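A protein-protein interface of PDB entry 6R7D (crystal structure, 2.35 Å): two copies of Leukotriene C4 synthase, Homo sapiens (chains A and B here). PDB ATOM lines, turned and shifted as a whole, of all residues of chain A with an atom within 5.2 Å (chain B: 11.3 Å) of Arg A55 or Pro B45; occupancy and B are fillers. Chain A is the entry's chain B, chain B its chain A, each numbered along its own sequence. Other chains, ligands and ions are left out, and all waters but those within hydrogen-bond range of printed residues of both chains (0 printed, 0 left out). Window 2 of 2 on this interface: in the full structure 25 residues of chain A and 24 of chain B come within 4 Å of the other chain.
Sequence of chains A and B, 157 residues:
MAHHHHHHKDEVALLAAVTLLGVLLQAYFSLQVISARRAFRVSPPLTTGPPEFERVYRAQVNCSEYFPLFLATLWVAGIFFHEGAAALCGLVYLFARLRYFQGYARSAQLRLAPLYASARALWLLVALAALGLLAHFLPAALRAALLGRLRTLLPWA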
ATOM      1  N   PRO A  51      -4.625  11.215   2.909  1.00  0.00           N
ATOM      2  CA  PRO A  51      -4.616  11.770   4.248  1.00  0.00           C
ATOM      3  C   PRO A  51      -3.756  13.019   4.444  1.00  0.00           C
ATOM      4  O   PRO A  51      -4.119  13.900   5.259  1.00  0.00           O
ATOM      5  CB  PRO A  51      -4.181  10.575   5.135  1.00  0.00           C
ATOM      6  CG  PRO A  51      -4.558   9.345   4.353  1.00  0.00           C
ATOM      7  CD  PRO A  51      -4.307   9.766   2.902  1.00  0.00           C
ATOM      8  N   GLU A  52      -2.573  13.039   3.845  1.00  0.00           N
ATOM      9  CA  GLU A  52      -1.579  14.107   4.080  1.00  0.00           C
ATOM     10  C   GLU A  52      -2.137  15.484   3.608  1.00  0.00           C
ATOM     11  O   GLU A  52      -1.976  16.557   4.234  1.00  0.00           O
ATOM     12  CB  GLU A  52      -0.237  13.785   3.331  1.00  0.00           C
ATOM     13  CG  GLU A  52       0.698  12.696   3.735  1.00  0.00           C
ATOM     14  CD  GLU A  52       0.123  11.229   3.721  1.00  0.00           C
ATOM     15  OE1 GLU A  52      -0.745  10.769   2.873  1.00  0.00           O
ATOM     16  OE2 GLU A  52       0.541  10.606   4.753  1.00  0.00           O
ATOM     17  N   PHE A  53      -2.914  15.405   2.552  1.00  0.00           N
ATOM     18  CA  PHE A  53      -3.723  16.575   2.097  1.00  0.00           C
ATOM     19  C   PHE A  53      -4.883  16.942   3.016  1.00  0.00           C
ATOM     20  O   PHE A  53      -5.035  18.065   3.409  1.00  0.00           O
ATOM     21  CB  PHE A  53      -4.258  16.367   0.682  1.00  0.00           C
ATOM     22  CG  PHE A  53      -5.251  17.392   0.333  1.00  0.00           C
ATOM     23  CD1 PHE A  53      -4.837  18.665  -0.019  1.00  0.00           C
ATOM     24  CD2 PHE A  53      -6.565  17.133   0.500  1.00  0.00           C
ATOM     25  CE1 PHE A  53      -5.794  19.663  -0.239  1.00  0.00           C
ATOM     26  CE2 PHE A  53      -7.524  18.113   0.256  1.00  0.00           C
ATOM     27  CZ  PHE A  53      -7.133  19.405  -0.053  1.00  0.00           C
ATOM     28  N   GLU A  54      -5.647  15.934   3.384  1.00  0.00           N
ATOM     29  CA  GLU A  54      -6.806  16.139   4.238  1.00  0.00           C
ATOM     30  C   GLU A  54      -6.456  16.780   5.610  1.00  0.00           C
ATOM     31  O   GLU A  54      -7.244  17.580   6.088  1.00  0.00           O
ATOM     32  CB  GLU A  54      -7.652  14.866   4.468  1.00  0.00           C
ATOM     33  CG  GLU A  54      -8.462  14.545   3.231  1.00  0.00           C
ATOM     34  CD  GLU A  54      -9.464  13.387   3.379  1.00  0.00           C
ATOM     35  OE1 GLU A  54      -9.666  12.809   4.490  1.00  0.00           O
ATOM     36  OE2 GLU A  54     -10.092  13.100   2.369  1.00  0.00           O
ATOM     37  N   ARG A  55      -5.337  16.408   6.208  1.00  0.00           N
ATOM     38  CA  ARG A  55      -4.980  16.919   7.463  1.00  0.00           C
ATOM     39  C   ARG A  55      -4.602  18.436   7.327  1.00  0.00           C
ATOM     40  O   ARG A  55      -4.922  19.225   8.212  1.00  0.00           O
ATOM     41  CB  ARG A  55      -3.854  16.122   8.059  1.00  0.00           C
ATOM     42  CG  ARG A  55      -4.264  14.667   8.465  1.00  0.00           C
ATOM     43  CD  ARG A  55      -3.241  14.071   9.460  1.00  0.00           C
ATOM     44  NE  ARG A  55      -1.879  14.107   8.884  1.00  0.00           N
ATOM     45  CZ  ARG A  55      -1.362  13.123   8.103  1.00  0.00           C
ATOM     46  NH1 ARG A  55      -2.083  12.078   7.762  1.00  0.00           N
ATOM     47  NH2 ARG A  55      -0.169  13.281   7.599  1.00  0.00           N
ATOM     48  N   VAL A  56      -3.882  18.788   6.276  1.00  0.00           N
ATOM     49  CA  VAL A  56      -3.476  20.178   6.045  1.00  0.00           C
ATOM     50  C   VAL A  56      -4.719  21.007   5.827  1.00  0.00           C
ATOM     51  O   VAL A  56      -4.874  22.100   6.378  1.00  0.00           O
ATOM     52  CB  VAL A  56      -2.466  20.233   4.870  1.00  0.00           C
ATOM     53  CG1 VAL A  56      -2.162  21.663   4.472  1.00  0.00           C
ATOM     54  CG2 VAL A  56      -1.082  19.577   5.280  1.00  0.00           C
ATOM     55  N   TYR A  57      -5.615  20.481   4.994  1.00  0.00           N
ATOM     56  CA  TYR A  57      -6.810  21.167   4.632  1.00  0.00           C
ATOM     57  C   TYR A  57      -7.689  21.369   5.843  1.00  0.00           C
ATOM     58  O   TYR A  57      -8.182  22.446   6.101  1.00  0.00           O
ATOM     59  CB  TYR A  57      -7.518  20.427   3.498  1.00  0.00           C
ATOM     60  CG  TYR A  57      -8.880  20.944   3.183  1.00  0.00           C
ATOM     61  CD1 TYR A  57      -9.084  22.096   2.402  1.00  0.00           C
ATOM     62  CD2 TYR A  57      -9.995  20.286   3.697  1.00  0.00           C
ATOM     63  CE1 TYR A  57     -10.384  22.598   2.226  1.00  0.00           C
ATOM     64  CE2 TYR A  57     -11.242  20.750   3.478  1.00  0.00           C
ATOM     65  CZ  TYR A  57     -11.403  21.948   2.797  1.00  0.00           C
ATOM     66  OH  TYR A  57     -12.711  22.252   2.521  1.00  0.00           O
ATOM     67  N   ARG A  58      -7.825  20.345   6.651  1.00  0.00           N
ATOM     68  CA  ARG A  58      -8.641  20.407   7.851  1.00  0.00           C
ATOM     69  C   ARG A  58      -8.062  21.398   8.870  1.00  0.00           C
ATOM     70  O   ARG A  58      -8.806  22.114   9.521  1.00  0.00           O
ATOM     71  CB  ARG A  58      -8.748  19.031   8.480  1.00  0.00           C
ATOM     72  CG  ARG A  58      -9.827  18.146   7.801  1.00  0.00           C
ATOM     73  CD  ARG A  58     -11.034  18.498   8.646  1.00  0.00           C
ATOM     74  NE  ARG A  58     -11.928  19.220   7.933  1.00  0.00           N
ATOM     75  CZ  ARG A  58     -12.864  20.044   8.447  1.00  0.00           C
ATOM     76  NH1 ARG A  58     -13.034  20.460   9.685  1.00  0.00           N
ATOM     77  NH2 ARG A  58     -13.606  20.594   7.521  1.00  0.00           N
ATOM     78  N   ALA A  59      -6.744  21.387   9.030  1.00  0.00           N
ATOM     79  CA  ALA A  59      -6.071  22.282   9.936  1.00  0.00           C
ATOM     80  C   ALA A  59      -6.410  23.723   9.580  1.00  0.00           C
ATOM     81  O   ALA A  59      -6.746  24.531  10.451  1.00  0.00           O
ATOM     82  CB  ALA A  59      -4.581  22.066   9.872  1.00  0.00           C
ATOM     83  N   GLN A  60      -6.318  24.047   8.304  1.00  0.00           N
ATOM     84  CA  GLN A  60      -6.636  25.373   7.796  1.00  0.00           C
ATOM     85  C   GLN A  60      -8.089  25.707   8.021  1.00  0.00           C
ATOM     86  O   GLN A  60      -8.402  26.735   8.573  1.00  0.00           O
ATOM     87  CB  GLN A  60      -6.274  25.471   6.333  1.00  0.00           C
ATOM     88  CG  GLN A  60      -6.514  26.801   5.698  1.00  0.00           C
ATOM     89  CD  GLN A  60      -7.727  26.890   4.896  1.00  0.00           C
ATOM     90  OE1 GLN A  60      -7.975  26.066   4.083  1.00  0.00           O
ATOM     91  NE2 GLN A  60      -8.561  27.854   5.170  1.00  0.00           N
ATOM     92  N   TYR A 104      -0.562  18.848  12.913  1.00  0.00           N
ATOM     93  CA  TYR A 104      -1.609  18.134  12.247  1.00  0.00           C
ATOM     94  C   TYR A 104      -1.081  17.688  10.925  1.00  0.00           C
ATOM     95  O   TYR A 104      -1.453  16.572  10.488  1.00  0.00           O
ATOM     96  CB  TYR A 104      -2.885  19.028  12.049  1.00  0.00           C
ATOM     97  CG  TYR A 104      -4.230  18.365  11.883  1.00  0.00           C
ATOM     98  CD1 TYR A 104      -4.386  16.962  11.671  1.00  0.00           C
ATOM     99  CD2 TYR A 104      -5.391  19.116  11.951  1.00  0.00           C
ATOM    100  CE1 TYR A 104      -5.639  16.401  11.492  1.00  0.00           C
ATOM    101  CE2 TYR A 104      -6.610  18.547  11.765  1.00  0.00           C
ATOM    102  CZ  TYR A 104      -6.710  17.139  11.567  1.00  0.00           C
ATOM    103  OH  TYR A 104      -7.964  16.618  11.462  1.00  0.00           O
ATOM    104  N   ALA A 105      -0.309  18.557  10.231  1.00  0.00           N
ATOM    105  CA  ALA A 105       0.252  18.186   8.908  1.00  0.00           C
ATOM    106  C   ALA A 105       0.967  16.804   9.041  1.00  0.00           C
ATOM    107  O   ALA A 105       0.832  15.918   8.173  1.00  0.00           O
ATOM    108  CB  ALA A 105       1.200  19.262   8.381  1.00  0.00           C
ATOM    109  N   ARG A 106       1.719  16.649  10.109  1.00  0.00           N
ATOM    110  CA  ARG A 106       2.531  15.434  10.361  1.00  0.00           C
ATOM    111  C   ARG A 106       1.589  14.291  10.750  1.00  0.00           C
ATOM    112  O   ARG A 106       1.659  13.275  10.142  1.00  0.00           O
ATOM    113  CB  ARG A 106       3.654  15.694  11.372  1.00  0.00           C
ATOM    114  CG  ARG A 106       4.648  16.749  10.907  1.00  0.00           C
ATOM    115  CD  ARG A 106       5.545  17.215  12.052  1.00  0.00           C
ATOM    116  NE  ARG A 106       6.305  16.052  12.541  1.00  0.00           N
ATOM    117  CZ  ARG A 106       7.063  15.950  13.640  1.00  0.00           C
ATOM    118  NH1 ARG A 106       7.157  16.955  14.498  1.00  0.00           N
ATOM    119  NH2 ARG A 106       7.717  14.811  13.907  1.00  0.00           N
ATOM    120  N   SER A 107       0.666  14.482  11.712  1.00  0.00           N
ATOM    121  CA  SER A 107      -0.374  13.438  12.043  1.00  0.00           C
ATOM    122  C   SER A 107      -1.465  14.028  12.945  1.00  0.00           C
ATOM    123  O   SER A 107      -1.250  15.056  13.634  1.00  0.00           O
ATOM    124  CB  SER A 107       0.271  12.249  12.804  1.00  0.00           C
ATOM    125  OG  SER A 107       0.457  12.621  14.169  1.00  0.00           O
ATOM    126  N   ALA A 108      -2.616  13.359  12.908  1.00  0.00           N
ATOM    127  CA  ALA A 108      -3.688  13.500  13.784  1.00  0.00           C
ATOM    128  C   ALA A 108      -3.341  13.641  15.229  1.00  0.00           C
ATOM    129  O   ALA A 108      -3.763  14.654  15.940  1.00  0.00           O
ATOM    130  CB  ALA A 108      -4.846  12.515  13.554  1.00  0.00           C
ATOM    131  N   VAL B  33     -20.021  18.197  19.120  1.00  0.00           N
ATOM    132  CA  VAL B  33     -19.361  17.572  18.006  1.00  0.00           C
ATOM    133  C   VAL B  33     -18.296  16.595  18.482  1.00  0.00           C
ATOM    134  O   VAL B  33     -18.224  15.474  17.960  1.00  0.00           O
ATOM    135  CB  VAL B  33     -18.823  18.567  16.954  1.00  0.00           C
ATOM    136  CG1 VAL B  33     -18.012  17.838  15.879  1.00  0.00           C
ATOM    137  CG2 VAL B  33     -19.972  19.322  16.286  1.00  0.00           C
ATOM    138  N   ARG B  37     -18.294  12.682  17.767  1.00  0.00           N
ATOM    139  CA  ARG B  37     -17.152  11.974  17.215  1.00  0.00           C
ATOM    140  C   ARG B  37     -16.806  10.692  18.041  1.00  0.00           C
ATOM    141  O   ARG B  37     -16.335   9.732  17.457  1.00  0.00           O
ATOM    142  CB  ARG B  37     -15.923  12.840  17.093  1.00  0.00           C
ATOM    143  CG  ARG B  37     -15.997  13.922  15.986  1.00  0.00           C
ATOM    144  CD  ARG B  37     -14.641  14.633  15.778  1.00  0.00           C
ATOM    145  NE  ARG B  37     -14.688  15.449  14.586  1.00  0.00           N
ATOM    146  CZ  ARG B  37     -14.471  15.095  13.348  1.00  0.00           C
ATOM    147  NH1 ARG B  37     -14.278  13.779  12.977  1.00  0.00           N
ATOM    148  NH2 ARG B  37     -14.539  15.994  12.398  1.00  0.00           N
ATOM    149  N   ARG B  41     -17.550   7.156  16.588  1.00  0.00           N
ATOM    150  CA  ARG B  41     -16.189   6.794  16.183  1.00  0.00           C
ATOM    151  C   ARG B  41     -15.780   7.396  14.833  1.00  0.00           C
ATOM    152  O   ARG B  41     -15.242   6.697  13.989  1.00  0.00           O
ATOM    153  CB  ARG B  41     -15.992   5.261  16.213  1.00  0.00           C
ATOM    154  CG  ARG B  41     -16.141   4.628  17.600  1.00  0.00           C
ATOM    155  CD  ARG B  41     -15.833   3.123  17.565  1.00  0.00           C
ATOM    156  NE  ARG B  41     -15.917   2.472  18.893  1.00  0.00           N
ATOM    157  CZ  ARG B  41     -14.968   2.479  19.844  1.00  0.00           C
ATOM    158  NH1 ARG B  41     -13.811   3.129  19.673  1.00  0.00           N
ATOM    159  NH2 ARG B  41     -15.174   1.839  20.998  1.00  0.00           N
ATOM    160  N   VAL B  42     -15.852   8.722  14.728  1.00  0.00           N
ATOM    161  CA  VAL B  42     -15.349   9.469  13.527  1.00  0.00           C
ATOM    162  C   VAL B  42     -14.161  10.337  13.888  1.00  0.00           C
ATOM    163  O   VAL B  42     -14.252  11.412  14.517  1.00  0.00           O
ATOM    164  CB  VAL B  42     -16.464  10.309  12.892  1.00  0.00           C
ATOM    165  CG1 VAL B  42     -16.028  10.889  11.575  1.00  0.00           C
ATOM    166  CG2 VAL B  42     -17.708   9.466  12.729  1.00  0.00           C
ATOM    167  N   SER B  43     -13.009   9.902  13.464  1.00  0.00           N
ATOM    168  CA  SER B  43     -11.728  10.441  13.877  1.00  0.00           C
ATOM    169  C   SER B  43     -11.390  11.504  12.896  1.00  0.00           C
ATOM    170  O   SER B  43     -11.361  11.272  11.701  1.00  0.00           O
ATOM    171  CB  SER B  43     -10.620   9.353  13.745  1.00  0.00           C
ATOM    172  OG  SER B  43     -10.728   8.440  14.829  1.00  0.00           O
ATOM    173  N   PRO B  44     -10.979  12.672  13.377  1.00  0.00           N
ATOM    174  CA  PRO B  44     -10.371  13.649  12.458  1.00  0.00           C
ATOM    175  C   PRO B  44      -9.254  13.022  11.693  1.00  0.00           C
ATOM    176  O   PRO B  44      -8.483  12.302  12.305  1.00  0.00           O
ATOM    177  CB  PRO B  44      -9.833  14.715  13.434  1.00  0.00           C
ATOM    178  CG  PRO B  44     -10.803  14.627  14.600  1.00  0.00           C
ATOM    179  CD  PRO B  44     -11.024  13.165  14.778  1.00  0.00           C
ATOM    180  N   PRO B  45      -9.048  13.334  10.418  1.00  0.00           N
ATOM    181  CA  PRO B  45      -9.666  14.473   9.693  1.00  0.00           C
ATOM    182  C   PRO B  45     -11.025  14.185   8.970  1.00  0.00           C
ATOM    183  O   PRO B  45     -11.475  14.983   8.126  1.00  0.00           O
ATOM    184  CB  PRO B  45      -8.573  14.833   8.662  1.00  0.00           C
ATOM    185  CG  PRO B  45      -7.894  13.476   8.358  1.00  0.00           C
ATOM    186  CD  PRO B  45      -7.916  12.738   9.666  1.00  0.00           C
ATOM    187  N   LEU B  46     -11.637  13.038   9.256  1.00  0.00           N
ATOM    188  CA  LEU B  46     -12.869  12.652   8.578  1.00  0.00           C
ATOM    189  C   LEU B  46     -13.991  13.574   9.019  1.00  0.00           C
ATOM    190  O   LEU B  46     -14.111  13.842  10.210  1.00  0.00           O
ATOM    191  CB  LEU B  46     -13.257  11.182   8.853  1.00  0.00           C
ATOM    192  CG  LEU B  46     -13.056  10.082   7.766  1.00  0.00           C
ATOM    193  CD1 LEU B  46     -11.785  10.330   6.923  1.00  0.00           C
ATOM    194  CD2 LEU B  46     -13.066   8.736   8.470  1.00  0.00           C
ATOM    195  N   THR B  47     -14.789  13.998   8.052  1.00  0.00           N
ATOM    196  CA  THR B  47     -15.962  14.736   8.295  1.00  0.00           C
ATOM    197  C   THR B  47     -17.252  14.045   7.862  1.00  0.00           C
ATOM    198  O   THR B  47     -18.298  14.612   8.029  1.00  0.00           O
ATOM    199  CB  THR B  47     -15.878  16.155   7.610  1.00  0.00           C
ATOM    200  OG1 THR B  47     -16.004  15.992   6.209  1.00  0.00           O
ATOM    201  CG2 THR B  47     -14.594  16.799   7.880  1.00  0.00           C
ATOM    202  N   THR B  48     -17.191  12.791   7.477  1.00  0.00           N
ATOM    203  CA  THR B  48     -18.366  11.985   7.053  1.00  0.00           C
ATOM    204  C   THR B  48     -18.464  10.757   7.948  1.00  0.00           C
ATOM    205  O   THR B  48     -17.499  10.398   8.599  1.00  0.00           O
ATOM    206  CB  THR B  48     -18.264  11.566   5.558  1.00  0.00           C
ATOM    207  OG1 THR B  48     -17.008  10.961   5.366  1.00  0.00           O
ATOM    208  CG2 THR B  48     -18.406  12.830   4.614  1.00  0.00           C
ATOM    209  N   GLY B  49     -19.654  10.193   8.042  1.00  0.00           N
ATOM    210  CA  GLY B  49     -19.938   9.178   8.993  1.00  0.00           C
ATOM    211  C   GLY B  49     -21.413   9.053   9.108  1.00  0.00           C
ATOM    212  O   GLY B  49     -22.092   9.227   8.104  1.00  0.00           O
ATOM    213  N   PHE B  53     -24.074  11.611  13.300  1.00  0.00           N
ATOM    214  CA  PHE B  53     -22.870  12.405  13.357  1.00  0.00           C
ATOM    215  C   PHE B  53     -22.880  13.568  12.330  1.00  0.00           C
ATOM    216  O   PHE B  53     -22.600  14.691  12.673  1.00  0.00           O
ATOM    217  CB  PHE B  53     -21.606  11.528  13.138  1.00  0.00           C
ATOM    218  CG  PHE B  53     -20.381  12.365  12.854  1.00  0.00           C
ATOM    219  CD1 PHE B  53     -19.786  13.030  13.906  1.00  0.00           C
ATOM    220  CD2 PHE B  53     -19.988  12.644  11.561  1.00  0.00           C
ATOM    221  CE1 PHE B  53     -18.763  13.917  13.683  1.00  0.00           C
ATOM    222  CE2 PHE B  53     -18.975  13.580  11.310  1.00  0.00           C
ATOM    223  CZ  PHE B  53     -18.367  14.251  12.392  1.00  0.00           C
ATOM    224  N   GLU B  54     -23.214  13.273  11.074  1.00  0.00           N
ATOM    225  CA  GLU B  54     -23.256  14.309  10.041  1.00  0.00           C
ATOM    226  C   GLU B  54     -24.171  15.475  10.317  1.00  0.00           C
ATOM    227  O   GLU B  54     -23.805  16.598   9.983  1.00  0.00           O
ATOM    228  CB  GLU B  54     -23.553  13.775   8.645  1.00  0.00           C
ATOM    229  CG  GLU B  54     -22.357  13.010   8.078  1.00  0.00           C
ATOM    230  CD  GLU B  54     -22.464  12.598   6.612  1.00  0.00           C
ATOM    231  OE1 GLU B  54     -23.471  12.905   5.896  1.00  0.00           O
ATOM    232  OE2 GLU B  54     -21.514  11.908   6.171  1.00  0.00           O
ATOM    233  N   TYR B  57     -22.512  17.624  13.102  1.00  0.00           N
ATOM    234  CA  TYR B  57     -21.387  18.253  12.540  1.00  0.00           C
ATOM    235  C   TYR B  57     -21.820  19.384  11.635  1.00  0.00           C
ATOM    236  O   TYR B  57     -21.275  20.486  11.704  1.00  0.00           O
ATOM    237  CB  TYR B  57     -20.488  17.229  11.822  1.00  0.00           C
ATOM    238  CG  TYR B  57     -19.362  17.832  11.012  1.00  0.00           C
ATOM    239  CD1 TYR B  57     -18.200  18.289  11.613  1.00  0.00           C
ATOM    240  CD2 TYR B  57     -19.510  17.999   9.627  1.00  0.00           C
ATOM    241  CE1 TYR B  57     -17.210  18.896  10.845  1.00  0.00           C
ATOM    242  CE2 TYR B  57     -18.533  18.532   8.862  1.00  0.00           C
ATOM    243  CZ  TYR B  57     -17.437  19.054   9.487  1.00  0.00           C
ATOM    244  OH  TYR B  57     -16.435  19.525   8.688  1.00  0.00           O
ATOM    245  N   VAL B  61     -21.073  23.430  11.864  1.00  0.00           N
ATOM    246  CA  VAL B  61     -20.451  24.165  10.781  1.00  0.00           C
ATOM    247  C   VAL B  61     -21.313  25.312  10.320  1.00  0.00           C
ATOM    248  O   VAL B  61     -20.797  26.399  10.166  1.00  0.00           O
ATOM    249  CB  VAL B  61     -19.956  23.272   9.591  1.00  0.00           C
ATOM    250  CG1 VAL B  61     -19.336  24.056   8.411  1.00  0.00           C
ATOM    251  CG2 VAL B  61     -18.947  22.221  10.061  1.00  0.00           C
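The side-chain hydroxyl of Tyr B57 is in hydrogen-bond range of the guanidinium group of Arg A58 (3.2 Å).
Positions printed for both chains: 53, 54 and 57. Of the 8 pairs that touch across the chains among the printed residues, none has its exchanged pair printed and touching as well.
Glu A54 touches Pro B45. Arg A55 touches Pro B45. O of Pro B45 touches CD of Arg A58, at 3.6 Å. NE of Arg A58 touches CG2 of Thr B47 (3.6 Å). CB of Pro B44 touches OH of Tyr A104, 3.3 Å away. OH of Tyr A104 touches CA of Pro B45, at 3.3 Å. Pro B44 touches Ala A108.
Hydrophobic or aromatic side chains of chain B that line the printed part of chain A: Pro B44, Pro B45 and Tyr B57. Printed residues of chain A that touch a printed residue of chain B: Glu A54, Arg A55, Arg A58, Tyr A104 and Ala A108. Hydrophobic or aromatic side chains of chain A that line the printed part of chain B: Tyr A104 and Ala A108. Among the printed residues, 8 pairs touch across the chains.
Arg A55 touches one residue of chain B. Printed residues of chain A within 4 Å of Pro B45: Glu A54, Arg A55, Arg A58 and Tyr A104. No residue of chain B comes within 4 Å of Glu A52. No residue of chain B comes within 4 Å of Phe A53. No residue of chain B comes within 4 Å of Val A56. Printed residues of chain B within 4 Å of Arg A58: Pro B45, Thr B47 and Tyr B57. No residue of chain B comes within 4 Å of Ala A59. No residue of chain B comes within 4 Å of Ala A105. Of chain B, only Pro B44 (3.9 Å) comes within 4 Å of Ala A108. Printed residues of chain A within 4 Å of Thr B47: Arg A58 (3.6 Å). Of the printed residues of chain B, Glu A54 touches Pro B45. Arg A106 touches none of the printed residues of chain B. Gln A60 touches none of the printed residues of chain B. The nearest residue of chain B that does not touch Arg A55 is Pro B44 (6.2 Å).
The guanidinium group (NH2) of Arg A55 lies within hydrogen-bond range of the backbone carbonyl oxygen (O) of Arg A106 (3.1 Å). The backbone carbonyl oxygen of Tyr A104 sits at hydrogen-bond distance from the guanidinium group of Arg A55 (3.0 Å). NH2 of Arg A55 is in salt-bridge range of OE2 of Glu A52, at 3.97 Å. The guanidinium group of Arg A55 sits at hydrogen-bond distance from the backbone carbonyl oxygen of Ala A105 (2.9 Å).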
